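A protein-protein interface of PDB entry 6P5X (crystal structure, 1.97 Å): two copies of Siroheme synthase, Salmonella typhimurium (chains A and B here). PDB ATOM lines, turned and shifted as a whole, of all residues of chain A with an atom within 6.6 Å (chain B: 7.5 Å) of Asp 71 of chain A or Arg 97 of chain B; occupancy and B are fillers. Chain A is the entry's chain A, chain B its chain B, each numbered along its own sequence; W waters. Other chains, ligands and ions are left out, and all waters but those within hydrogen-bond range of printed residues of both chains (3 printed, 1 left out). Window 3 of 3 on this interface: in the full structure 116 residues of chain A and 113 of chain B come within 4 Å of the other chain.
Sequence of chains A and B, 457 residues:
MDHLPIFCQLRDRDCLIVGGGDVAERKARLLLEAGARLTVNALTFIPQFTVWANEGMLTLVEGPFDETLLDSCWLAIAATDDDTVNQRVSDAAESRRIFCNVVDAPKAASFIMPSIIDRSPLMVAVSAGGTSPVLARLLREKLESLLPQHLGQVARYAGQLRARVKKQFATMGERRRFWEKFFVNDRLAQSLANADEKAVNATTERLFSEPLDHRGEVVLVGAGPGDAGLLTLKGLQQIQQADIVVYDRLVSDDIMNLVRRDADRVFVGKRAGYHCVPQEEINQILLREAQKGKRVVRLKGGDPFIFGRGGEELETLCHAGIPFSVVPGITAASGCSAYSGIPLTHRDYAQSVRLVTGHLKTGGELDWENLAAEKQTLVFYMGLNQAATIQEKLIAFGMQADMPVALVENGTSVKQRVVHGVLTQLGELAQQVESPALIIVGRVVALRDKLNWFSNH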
ATOM      1  N   ASP A  14      -3.120 -28.564  10.066  1.00  0.00           N
ATOM      2  CA  ASP A  14      -3.663 -27.403  10.766  1.00  0.00           C
ATOM      3  C   ASP A  14      -3.855 -26.212   9.833  1.00  0.00           C
ATOM      4  O   ASP A  14      -2.938 -25.827   9.094  1.00  0.00           O
ATOM      5  CB  ASP A  14      -2.733 -27.001  11.915  1.00  0.00           C
ATOM      6  CG  ASP A  14      -2.675 -28.040  13.017  1.00  0.00           C
ATOM      7  OD1 ASP A  14      -3.293 -29.109  12.863  1.00  0.00           O
ATOM      8  OD2 ASP A  14      -2.007 -27.777  14.036  1.00  0.00           O
ATOM      9  N   GLU A  67      -1.845 -14.493  17.406  1.00  0.00           N
ATOM     10  CA  GLU A  67      -0.989 -14.894  16.298  1.00  0.00           C
ATOM     11  C   GLU A  67      -0.230 -16.185  16.589  1.00  0.00           C
ATOM     12  O   GLU A  67       0.230 -16.836  15.638  1.00  0.00           O
ATOM     13  CB  GLU A  67      -0.024 -13.770  15.921  1.00  0.00           C
ATOM     14  CG  GLU A  67       1.138 -13.573  16.853  1.00  0.00           C
ATOM     15  CD  GLU A  67       2.045 -12.430  16.402  1.00  0.00           C
ATOM     16  OE1 GLU A  67       2.194 -12.225  15.179  1.00  0.00           O
ATOM     17  OE2 GLU A  67       2.605 -11.731  17.275  1.00  0.00           O
ATOM     18  N   THR A  68      -0.129 -16.605  17.856  1.00  0.00           N
ATOM     19  CA  THR A  68       0.500 -17.901  18.112  1.00  0.00           C
ATOM     20  C   THR A  68      -0.325 -19.060  17.558  1.00  0.00           C
ATOM     21  O   THR A  68       0.208 -20.165  17.419  1.00  0.00           O
ATOM     22  CB  THR A  68       0.777 -18.116  19.608  1.00  0.00           C
ATOM     23  OG1 THR A  68      -0.432 -18.364  20.335  1.00  0.00           O
ATOM     24  CG2 THR A  68       1.510 -16.921  20.211  1.00  0.00           C
ATOM     25  N   LEU A  69      -1.601 -18.833  17.237  1.00  0.00           N
ATOM     26  CA  LEU A  69      -2.420 -19.863  16.597  1.00  0.00           C
ATOM     27  C   LEU A  69      -1.954 -20.170  15.184  1.00  0.00           C
ATOM     28  O   LEU A  69      -2.340 -21.202  14.623  1.00  0.00           O
ATOM     29  CB  LEU A  69      -3.883 -19.437  16.563  1.00  0.00           C
ATOM     30  CG  LEU A  69      -4.582 -19.385  17.922  1.00  0.00           C
ATOM     31  CD1 LEU A  69      -5.972 -18.812  17.783  1.00  0.00           C
ATOM     32  CD2 LEU A  69      -4.616 -20.778  18.535  1.00  0.00           C
ATOM     33  N   LEU A  70      -1.124 -19.305  14.600  1.00  0.00           N
ATOM     34  CA  LEU A  70      -0.538 -19.614  13.300  1.00  0.00           C
ATOM     35  C   LEU A  70       0.614 -20.606  13.384  1.00  0.00           C
ATOM     36  O   LEU A  70       0.989 -21.192  12.360  1.00  0.00           O
ATOM     37  CB  LEU A  70      -0.040 -18.338  12.635  1.00  0.00           C
ATOM     38  CG  LEU A  70      -1.155 -17.402  12.168  1.00  0.00           C
ATOM     39  CD1 LEU A  70      -0.536 -16.063  11.809  1.00  0.00           C
ATOM     40  CD2 LEU A  70      -1.847 -18.001  10.954  1.00  0.00           C
ATOM     41  N   ASP A  71       1.164 -20.836  14.576  1.00  0.00           N
ATOM     42  CA  ASP A  71       2.483 -21.456  14.666  1.00  0.00           C
ATOM     43  C   ASP A  71       2.545 -22.822  13.998  1.00  0.00           C
ATOM     44  O   ASP A  71       3.590 -23.191  13.454  1.00  0.00           O
ATOM     45  CB  ASP A  71       2.922 -21.581  16.123  1.00  0.00           C
ATOM     46  CG  ASP A  71       3.288 -20.237  16.739  1.00  0.00           C
ATOM     47  OD1 ASP A  71       3.282 -19.222  16.019  1.00  0.00           O
ATOM     48  OD2 ASP A  71       3.573 -20.198  17.946  1.00  0.00           O
ATOM     49  N   SER A  72       1.462 -23.596  14.028  1.00  0.00           N
ATOM     50  CA  SER A  72       1.498 -24.933  13.432  1.00  0.00           C
ATOM     51  C   SER A  72       0.751 -25.009  12.099  1.00  0.00           C
ATOM     52  O   SER A  72       0.452 -26.109  11.611  1.00  0.00           O
ATOM     53  CB  SER A  72       0.938 -25.968  14.411  1.00  0.00           C
ATOM     54  OG  SER A  72      -0.437 -25.717  14.677  1.00  0.00           O
ATOM     55  N   CYS A  73       0.492 -23.876  11.464  1.00  0.00           N
ATOM     56  CA  CYS A  73      -0.503 -23.833  10.401  1.00  0.00           C
ATOM     57  C   CYS A  73       0.124 -23.892   9.009  1.00  0.00           C
ATOM     58  O   CYS A  73       1.255 -23.451   8.783  1.00  0.00           O
ATOM     59  CB  CYS A  73      -1.381 -22.591  10.523  1.00  0.00           C
ATOM     60  SG  CYS A  73      -2.677 -22.795  11.776  1.00  0.00           S
ATOM     61  N   TRP A  74      -0.647 -24.454   8.076  1.00  0.00           N
ATOM     62  CA  TRP A  74      -0.270 -24.543   6.676  1.00  0.00           C
ATOM     63  C   TRP A  74      -0.983 -23.513   5.813  1.00  0.00           C
ATOM     64  O   TRP A  74      -0.486 -23.172   4.733  1.00  0.00           O
ATOM     65  CB  TRP A  74      -0.609 -25.941   6.134  1.00  0.00           C
ATOM     66  CG  TRP A  74       0.169 -27.102   6.699  1.00  0.00           C
ATOM     67  CD1 TRP A  74       0.090 -27.615   7.965  1.00  0.00           C
ATOM     68  CD2 TRP A  74       1.105 -27.915   5.994  1.00  0.00           C
ATOM     69  NE1 TRP A  74       0.920 -28.698   8.090  1.00  0.00           N
ATOM     70  CE2 TRP A  74       1.562 -28.904   6.893  1.00  0.00           C
ATOM     71  CE3 TRP A  74       1.588 -27.917   4.678  1.00  0.00           C
ATOM     72  CZ2 TRP A  74       2.502 -29.882   6.529  1.00  0.00           C
ATOM     73  CZ3 TRP A  74       2.539 -28.893   4.321  1.00  0.00           C
ATOM     74  CH2 TRP A  74       2.968 -29.864   5.239  1.00  0.00           C
ATOM     75  N   ARG A  96       5.717 -16.113   8.890  1.00  0.00           N
ATOM     76  CA  ARG A  96       5.867 -17.554   9.066  1.00  0.00           C
ATOM     77  C   ARG A  96       5.885 -18.330   7.746  1.00  0.00           C
ATOM     78  O   ARG A  96       5.926 -19.567   7.774  1.00  0.00           O
ATOM     79  CB  ARG A  96       4.744 -18.080   9.967  1.00  0.00           C
ATOM     80  CG  ARG A  96       4.751 -17.448  11.388  1.00  0.00           C
ATOM     81  CD  ARG A  96       3.447 -17.695  12.126  1.00  0.00           C
ATOM     82  NE  ARG A  96       3.569 -17.448  13.573  1.00  0.00           N
ATOM     83  CZ  ARG A  96       3.542 -16.240  14.125  1.00  0.00           C
ATOM     84  NH1 ARG A  96       3.426 -15.173  13.349  1.00  0.00           N
ATOM     85  NH2 ARG A  96       3.636 -16.093  15.449  1.00  0.00           N
ATOM     86  N   ARG A  97       5.848 -17.638   6.601  1.00  0.00           N
ATOM     87  CA  ARG A  97       5.750 -18.271   5.273  1.00  0.00           C
ATOM     88  C   ARG A  97       4.535 -19.197   5.172  1.00  0.00           C
ATOM     89  O   ARG A  97       4.597 -20.297   4.607  1.00  0.00           O
ATOM     90  CB  ARG A  97       7.054 -18.987   4.918  1.00  0.00           C
ATOM     91  CG  ARG A  97       8.224 -18.011   4.884  1.00  0.00           C
ATOM     92  CD  ARG A  97       9.570 -18.724   4.862  1.00  0.00           C
ATOM     93  NE  ARG A  97       9.726 -19.568   6.039  1.00  0.00           N
ATOM     94  CZ  ARG A  97      10.206 -19.145   7.202  1.00  0.00           C
ATOM     95  NH1 ARG A  97      10.590 -17.881   7.351  1.00  0.00           N
ATOM     96  NH2 ARG A  97      10.304 -19.991   8.215  1.00  0.00           N
ATOM     97  N   ILE A  98       3.401 -18.726   5.677  1.00  0.00           N
ATOM     98  CA  ILE A  98       2.128 -19.421   5.596  1.00  0.00           C
ATOM     99  C   ILE A  98       1.284 -18.725   4.541  1.00  0.00           C
ATOM    100  O   ILE A  98       0.965 -17.529   4.672  1.00  0.00           O
ATOM    101  CB  ILE A  98       1.389 -19.412   6.950  1.00  0.00           C
ATOM    102  CG1 ILE A  98       2.261 -20.078   8.031  1.00  0.00           C
ATOM    103  CG2 ILE A  98      -0.023 -20.056   6.788  1.00  0.00           C
ATOM    104  CD1 ILE A  98       1.700 -19.848   9.467  1.00  0.00           C
ATOM    105  N   CYS B  73      11.686 -21.125   2.503  1.00  0.00           N
ATOM    106  CA  CYS B  73      10.976 -21.494   1.282  1.00  0.00           C
ATOM    107  C   CYS B  73       9.472 -21.650   1.490  1.00  0.00           C
ATOM    108  O   CYS B  73       9.020 -22.227   2.483  1.00  0.00           O
ATOM    109  CB  CYS B  73      11.540 -22.794   0.704  1.00  0.00           C
ATOM    110  SG  CYS B  73      12.880 -22.524  -0.453  1.00  0.00           S
ATOM    111  N   TRP B  74       8.709 -21.170   0.509  1.00  0.00           N
ATOM    112  CA  TRP B  74       7.246 -21.232   0.499  1.00  0.00           C
ATOM    113  C   TRP B  74       6.694 -22.447  -0.230  1.00  0.00           C
ATOM    114  O   TRP B  74       5.567 -22.864   0.041  1.00  0.00           O
ATOM    115  CB  TRP B  74       6.660 -19.978  -0.168  1.00  0.00           C
ATOM    116  CG  TRP B  74       6.888 -18.699   0.572  1.00  0.00           C
ATOM    117  CD1 TRP B  74       8.070 -18.051   0.743  1.00  0.00           C
ATOM    118  CD2 TRP B  74       5.896 -17.900   1.222  1.00  0.00           C
ATOM    119  NE1 TRP B  74       7.889 -16.901   1.477  1.00  0.00           N
ATOM    120  CE2 TRP B  74       6.554 -16.776   1.766  1.00  0.00           C
ATOM    121  CE3 TRP B  74       4.511 -18.017   1.387  1.00  0.00           C
ATOM    122  CZ2 TRP B  74       5.879 -15.783   2.475  1.00  0.00           C
ATOM    123  CZ3 TRP B  74       3.842 -17.020   2.093  1.00  0.00           C
ATOM    124  CH2 TRP B  74       4.524 -15.924   2.623  1.00  0.00           C
ATOM    125  N   ASP B  91      10.023 -35.258   3.116  1.00  0.00           N
ATOM    126  CA  ASP B  91      10.006 -35.251   4.577  1.00  0.00           C
ATOM    127  C   ASP B  91      10.517 -33.929   5.136  1.00  0.00           C
ATOM    128  O   ASP B  91       9.977 -33.421   6.127  1.00  0.00           O
ATOM    129  CB  ASP B  91      10.842 -36.407   5.137  1.00  0.00           C
ATOM    130  CG  ASP B  91      10.220 -37.771   4.870  1.00  0.00           C
ATOM    131  OD1 ASP B  91       9.003 -37.843   4.599  1.00  0.00           O
ATOM    132  OD2 ASP B  91      10.966 -38.774   4.936  1.00  0.00           O
ATOM    133  N   ALA B  92      11.576 -33.372   4.542  1.00  0.00           N
ATOM    134  CA  ALA B  92      12.102 -32.108   5.034  1.00  0.00           C
ATOM    135  C   ALA B  92      11.074 -31.003   4.874  1.00  0.00           C
ATOM    136  O   ALA B  92      10.905 -30.167   5.774  1.00  0.00           O
ATOM    137  CB  ALA B  92      13.395 -31.746   4.307  1.00  0.00           C
ATOM    138  N   ALA B  93      10.357 -30.999   3.744  1.00  0.00           N
ATOM    139  CA  ALA B  93       9.336 -29.976   3.533  1.00  0.00           C
ATOM    140  C   ALA B  93       8.172 -30.150   4.499  1.00  0.00           C
ATOM    141  O   ALA B  93       7.644 -29.162   5.033  1.00  0.00           O
ATOM    142  CB  ALA B  93       8.844 -30.018   2.081  1.00  0.00           C
ATOM    143  N   GLU B  94       7.751 -31.393   4.737  1.00  0.00           N
ATOM    144  CA  GLU B  94       6.593 -31.608   5.596  1.00  0.00           C
ATOM    145  C   GLU B  94       6.877 -31.186   7.033  1.00  0.00           C
ATOM    146  O   GLU B  94       6.012 -30.601   7.698  1.00  0.00           O
ATOM    147  CB  GLU B  94       6.151 -33.067   5.555  1.00  0.00           C
ATOM    148  CG  GLU B  94       4.856 -33.259   6.346  1.00  0.00           C
ATOM    149  CD  GLU B  94       4.277 -34.648   6.225  1.00  0.00           C
ATOM    150  OE1 GLU B  94       5.004 -35.570   5.791  1.00  0.00           O
ATOM    151  OE2 GLU B  94       3.086 -34.815   6.566  1.00  0.00           O
ATOM    152  N   SER B  95       8.076 -31.479   7.533  1.00  0.00           N
ATOM    153  CA  SER B  95       8.434 -31.059   8.883  1.00  0.00           C
ATOM    154  C   SER B  95       8.468 -29.540   9.014  1.00  0.00           C
ATOM    155  O   SER B  95       8.350 -29.018  10.126  1.00  0.00           O
ATOM    156  CB  SER B  95       9.792 -31.643   9.271  1.00  0.00           C
ATOM    157  OG  SER B  95      10.827 -30.914   8.638  1.00  0.00           O
ATOM    158  N   ARG B  96       8.616 -28.825   7.902  1.00  0.00           N
ATOM    159  CA  ARG B  96       8.614 -27.367   7.889  1.00  0.00           C
ATOM    160  C   ARG B  96       7.264 -26.770   7.484  1.00  0.00           C
ATOM    161  O   ARG B  96       7.158 -25.546   7.385  1.00  0.00           O
ATOM    162  CB  ARG B  96       9.712 -26.877   6.939  1.00  0.00           C
ATOM    163  CG  ARG B  96      11.130 -26.909   7.519  1.00  0.00           C
ATOM    164  CD  ARG B  96      12.134 -26.785   6.388  1.00  0.00           C
ATOM    165  NE  ARG B  96      13.518 -26.781   6.880  1.00  0.00           N
ATOM    166  CZ  ARG B  96      14.195 -27.883   7.178  1.00  0.00           C
ATOM    167  NH1 ARG B  96      13.610 -29.069   7.041  1.00  0.00           N
ATOM    168  NH2 ARG B  96      15.455 -27.800   7.618  1.00  0.00           N
ATOM    169  N   ARG B  97       6.242 -27.601   7.241  1.00  0.00           N
ATOM    170  CA  ARG B  97       4.919 -27.144   6.785  1.00  0.00           C
ATOM    171  C   ARG B  97       5.031 -26.350   5.480  1.00  0.00           C
ATOM    172  O   ARG B  97       4.389 -25.314   5.309  1.00  0.00           O
ATOM    173  CB  ARG B  97       4.197 -26.327   7.864  1.00  0.00           C
ATOM    174  CG  ARG B  97       3.894 -27.121   9.145  1.00  0.00           C
ATOM    175  CD  ARG B  97       3.548 -26.228  10.342  1.00  0.00           C
ATOM    176  NE  ARG B  97       4.537 -25.162  10.554  1.00  0.00           N
ATOM    177  CZ  ARG B  97       5.654 -25.283  11.269  1.00  0.00           C
ATOM    178  NH1 ARG B  97       5.960 -26.436  11.866  1.00  0.00           N
ATOM    179  NH2 ARG B  97       6.476 -24.247  11.389  1.00  0.00           N
ATOM    180  N   ILE B  98       5.857 -26.842   4.558  1.00  0.00           N
ATOM    181  CA  ILE B  98       6.017 -26.266   3.221  1.00  0.00           C
ATOM    182  C   ILE B  98       5.325 -27.182   2.229  1.00  0.00           C
ATOM    183  O   ILE B  98       5.721 -28.345   2.071  1.00  0.00           O
ATOM    184  CB  ILE B  98       7.502 -26.122   2.851  1.00  0.00           C
ATOM    185  CG1 ILE B  98       8.237 -25.178   3.807  1.00  0.00           C
ATOM    186  CG2 ILE B  98       7.672 -25.755   1.355  1.00  0.00           C
ATOM    187  CD1 ILE B  98       9.742 -25.271   3.650  1.00  0.00           C
ATOM    188  N   PHE B  99       4.316 -26.663   1.525  1.00  0.00           N
ATOM    189  CA  PHE B  99       3.677 -27.481   0.508  1.00  0.00           C
ATOM    190  C   PHE B  99       4.699 -27.968  -0.499  1.00  0.00           C
ATOM    191  O   PHE B  99       5.572 -27.216  -0.956  1.00  0.00           O
ATOM    192  CB  PHE B  99       2.566 -26.721  -0.199  1.00  0.00           C
ATOM    193  CG  PHE B  99       1.310 -26.629   0.624  1.00  0.00           C
ATOM    194  CD1 PHE B  99       0.952 -25.451   1.265  1.00  0.00           C
ATOM    195  CD2 PHE B  99       0.519 -27.750   0.806  1.00  0.00           C
ATOM    196  CE1 PHE B  99      -0.201 -25.384   2.045  1.00  0.00           C
ATOM    197  CE2 PHE B  99      -0.633 -27.692   1.580  1.00  0.00           C
ATOM    198  CZ  PHE B  99      -0.986 -26.511   2.195  1.00  0.00           C
ATOM    199  N   CYS B 100       4.585 -29.240  -0.828  1.00  0.00           N
ATOM    200  CA  CYS B 100       5.634 -29.912  -1.574  1.00  0.00           C
ATOM    201  C   CYS B 100       5.002 -30.848  -2.583  1.00  0.00           C
ATOM    202  O   CYS B 100       4.046 -31.577  -2.271  1.00  0.00           O
ATOM    203  CB  CYS B 100       6.567 -30.679  -0.618  1.00  0.00           C
ATOM    204  SG  CYS B 100       7.925 -31.548  -1.457  1.00  0.00           S
ATOM    205  N   SER B 110       2.292 -33.012  -0.620  1.00  0.00           N
ATOM    206  CA  SER B 110       1.235 -32.226  -0.001  1.00  0.00           C
ATOM    207  C   SER B 110       0.515 -31.340  -1.010  1.00  0.00           C
ATOM    208  O   SER B 110      -0.500 -30.719  -0.657  1.00  0.00           O
ATOM    209  CB  SER B 110       1.793 -31.393   1.163  1.00  0.00           C
ATOM    210  OG  SER B 110       2.986 -30.720   0.790  1.00  0.00           O
HETATM  211  O   HOH W   1       6.087 -22.434   4.041  1.00  0.00           O
HETATM  212  O   HOH W   2       9.238 -22.231   5.436  1.00  0.00           O
HETATM  213  O   HOH W   3       3.886 -22.747   9.664  1.00  0.00           O
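OD2 of Asp 14 of chain A lies within hydrogen-bond range of OG of Ser 72 of chain A (2.7 Å).
The backbone carbonyl oxygen (O) of Asp 14 of chain A is in hydrogen-bond range of the backbone NH (N) of Trp 74 of chain A (2.9 Å).
The backbone carbonyl oxygen of Leu 69 of chain A sits at hydrogen-bond distance from the side-chain sulfur of Cys 73 of chain A, 3.3 Å away.
NE of Arg 96 of chain A is in salt-bridge range of OD1 of Asp 71 of chain A (3.0 Å).
The backbone NH (N) of Ile 98 of chain B lies within hydrogen-bond range of the backbone carbonyl oxygen (O) of Ala 93 of chain B (3.0 Å).
Among the printed residues, pairs that only touch across the chains: Asp 71 of chain A with Arg 97 of chain B (3.6 Å), Ser 72 of chain A with Arg 97 of chain B (3.3 Å), Cys 73 of chain A with Arg 97 of chain B (3.9 Å), Trp 74 of chain A with Glu 94 of chain B (3.8 Å), Trp 74 of chain A with Arg 97 of chain B (3.5 Å), Trp 74 of chain A with Ile 98 of chain B (3.9 Å), Trp 74 of chain A with Phe 99 of chain B (3.5 Å), Arg 97 of chain A with Cys 73 of chain B (3.98 Å), Arg 97 of chain A with Trp 74 of chain B (3.6 Å) and Ile 98 of chain A with Trp 74 of chain B (3.9 Å).
Of chain B, only Arg 97 (3.6 Å) comes within 4 Å of Asp 71 of chain A.
Of chain A, only Asp 71 (3.6 Å), Ser 72 (3.3 Å), Cys 73 (3.9 Å) and Trp 74 (3.5 Å) come within 4 Å of Arg 97 of chain B.
Printed residues of chain B within 4 Å of Arg 97 of chain A: Cys 73 and Trp 74.
Printed residues of chain A within 4 Å of Phe 99 of chain B: Trp 74.
Arg 96 of chain A touches none of the printed residues of chain B.
Ala 93 of chain B touches none of the printed residues of chain A.
The nearest residue of chain B that does not touch Asp 71 of chain A is Arg 96 of chain B (7.4 Å).
The nearest residue of chain A that does not touch Arg 97 of chain B is Arg 97 of chain A (5.1 Å).
Hydrophobic or aromatic side chains of chain B that line the printed part of chain A: Trp 74 and Phe 99.
Along chain B the printed residues that touch a printed residue of chain A span positions 73 to 99.
Among the printed residues, 10 pairs touch across the chains.
Among the printed residues, no Asp or Glu carboxylate lies within 4 Å of a Lys or Arg side-chain nitrogen of the other chain.
Cys 73 of chain A touches Arg 97 of chain B, and with the chains exchanged Arg 97 of chain A touches Cys 73 of chain B.
Trp 74 of chain A touches Arg 97 of chain B, and with the chains exchanged Arg 97 of chain A touches Trp 74 of chain B.
Trp 74 of chain A touches Ile 98 of chain B, and with the chains exchanged Ile 98 of chain A touches Trp 74 of chain B.
Positions printed for both chains: 73, 74, 96, 97 and 98.
Of the 10 pairs that touch across the chains among the printed residues, 6 have their exchanged pair printed and touching as well.
Water W3 lies within hydrogen-bond range of the guanidinium group of Arg 97 of chain B (2.7 Å) and the backbone carbonyl oxygen of Cys 73 of chain A (2.9 Å).
Water W1 bridges O of Arg 97 of chain A and O of Cys 73 of chain B.
Water W2 lies within hydrogen-bond range of NE of Arg 97 of chain A (2.8 Å) and O of Cys 73 of chain B (3.0 Å).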
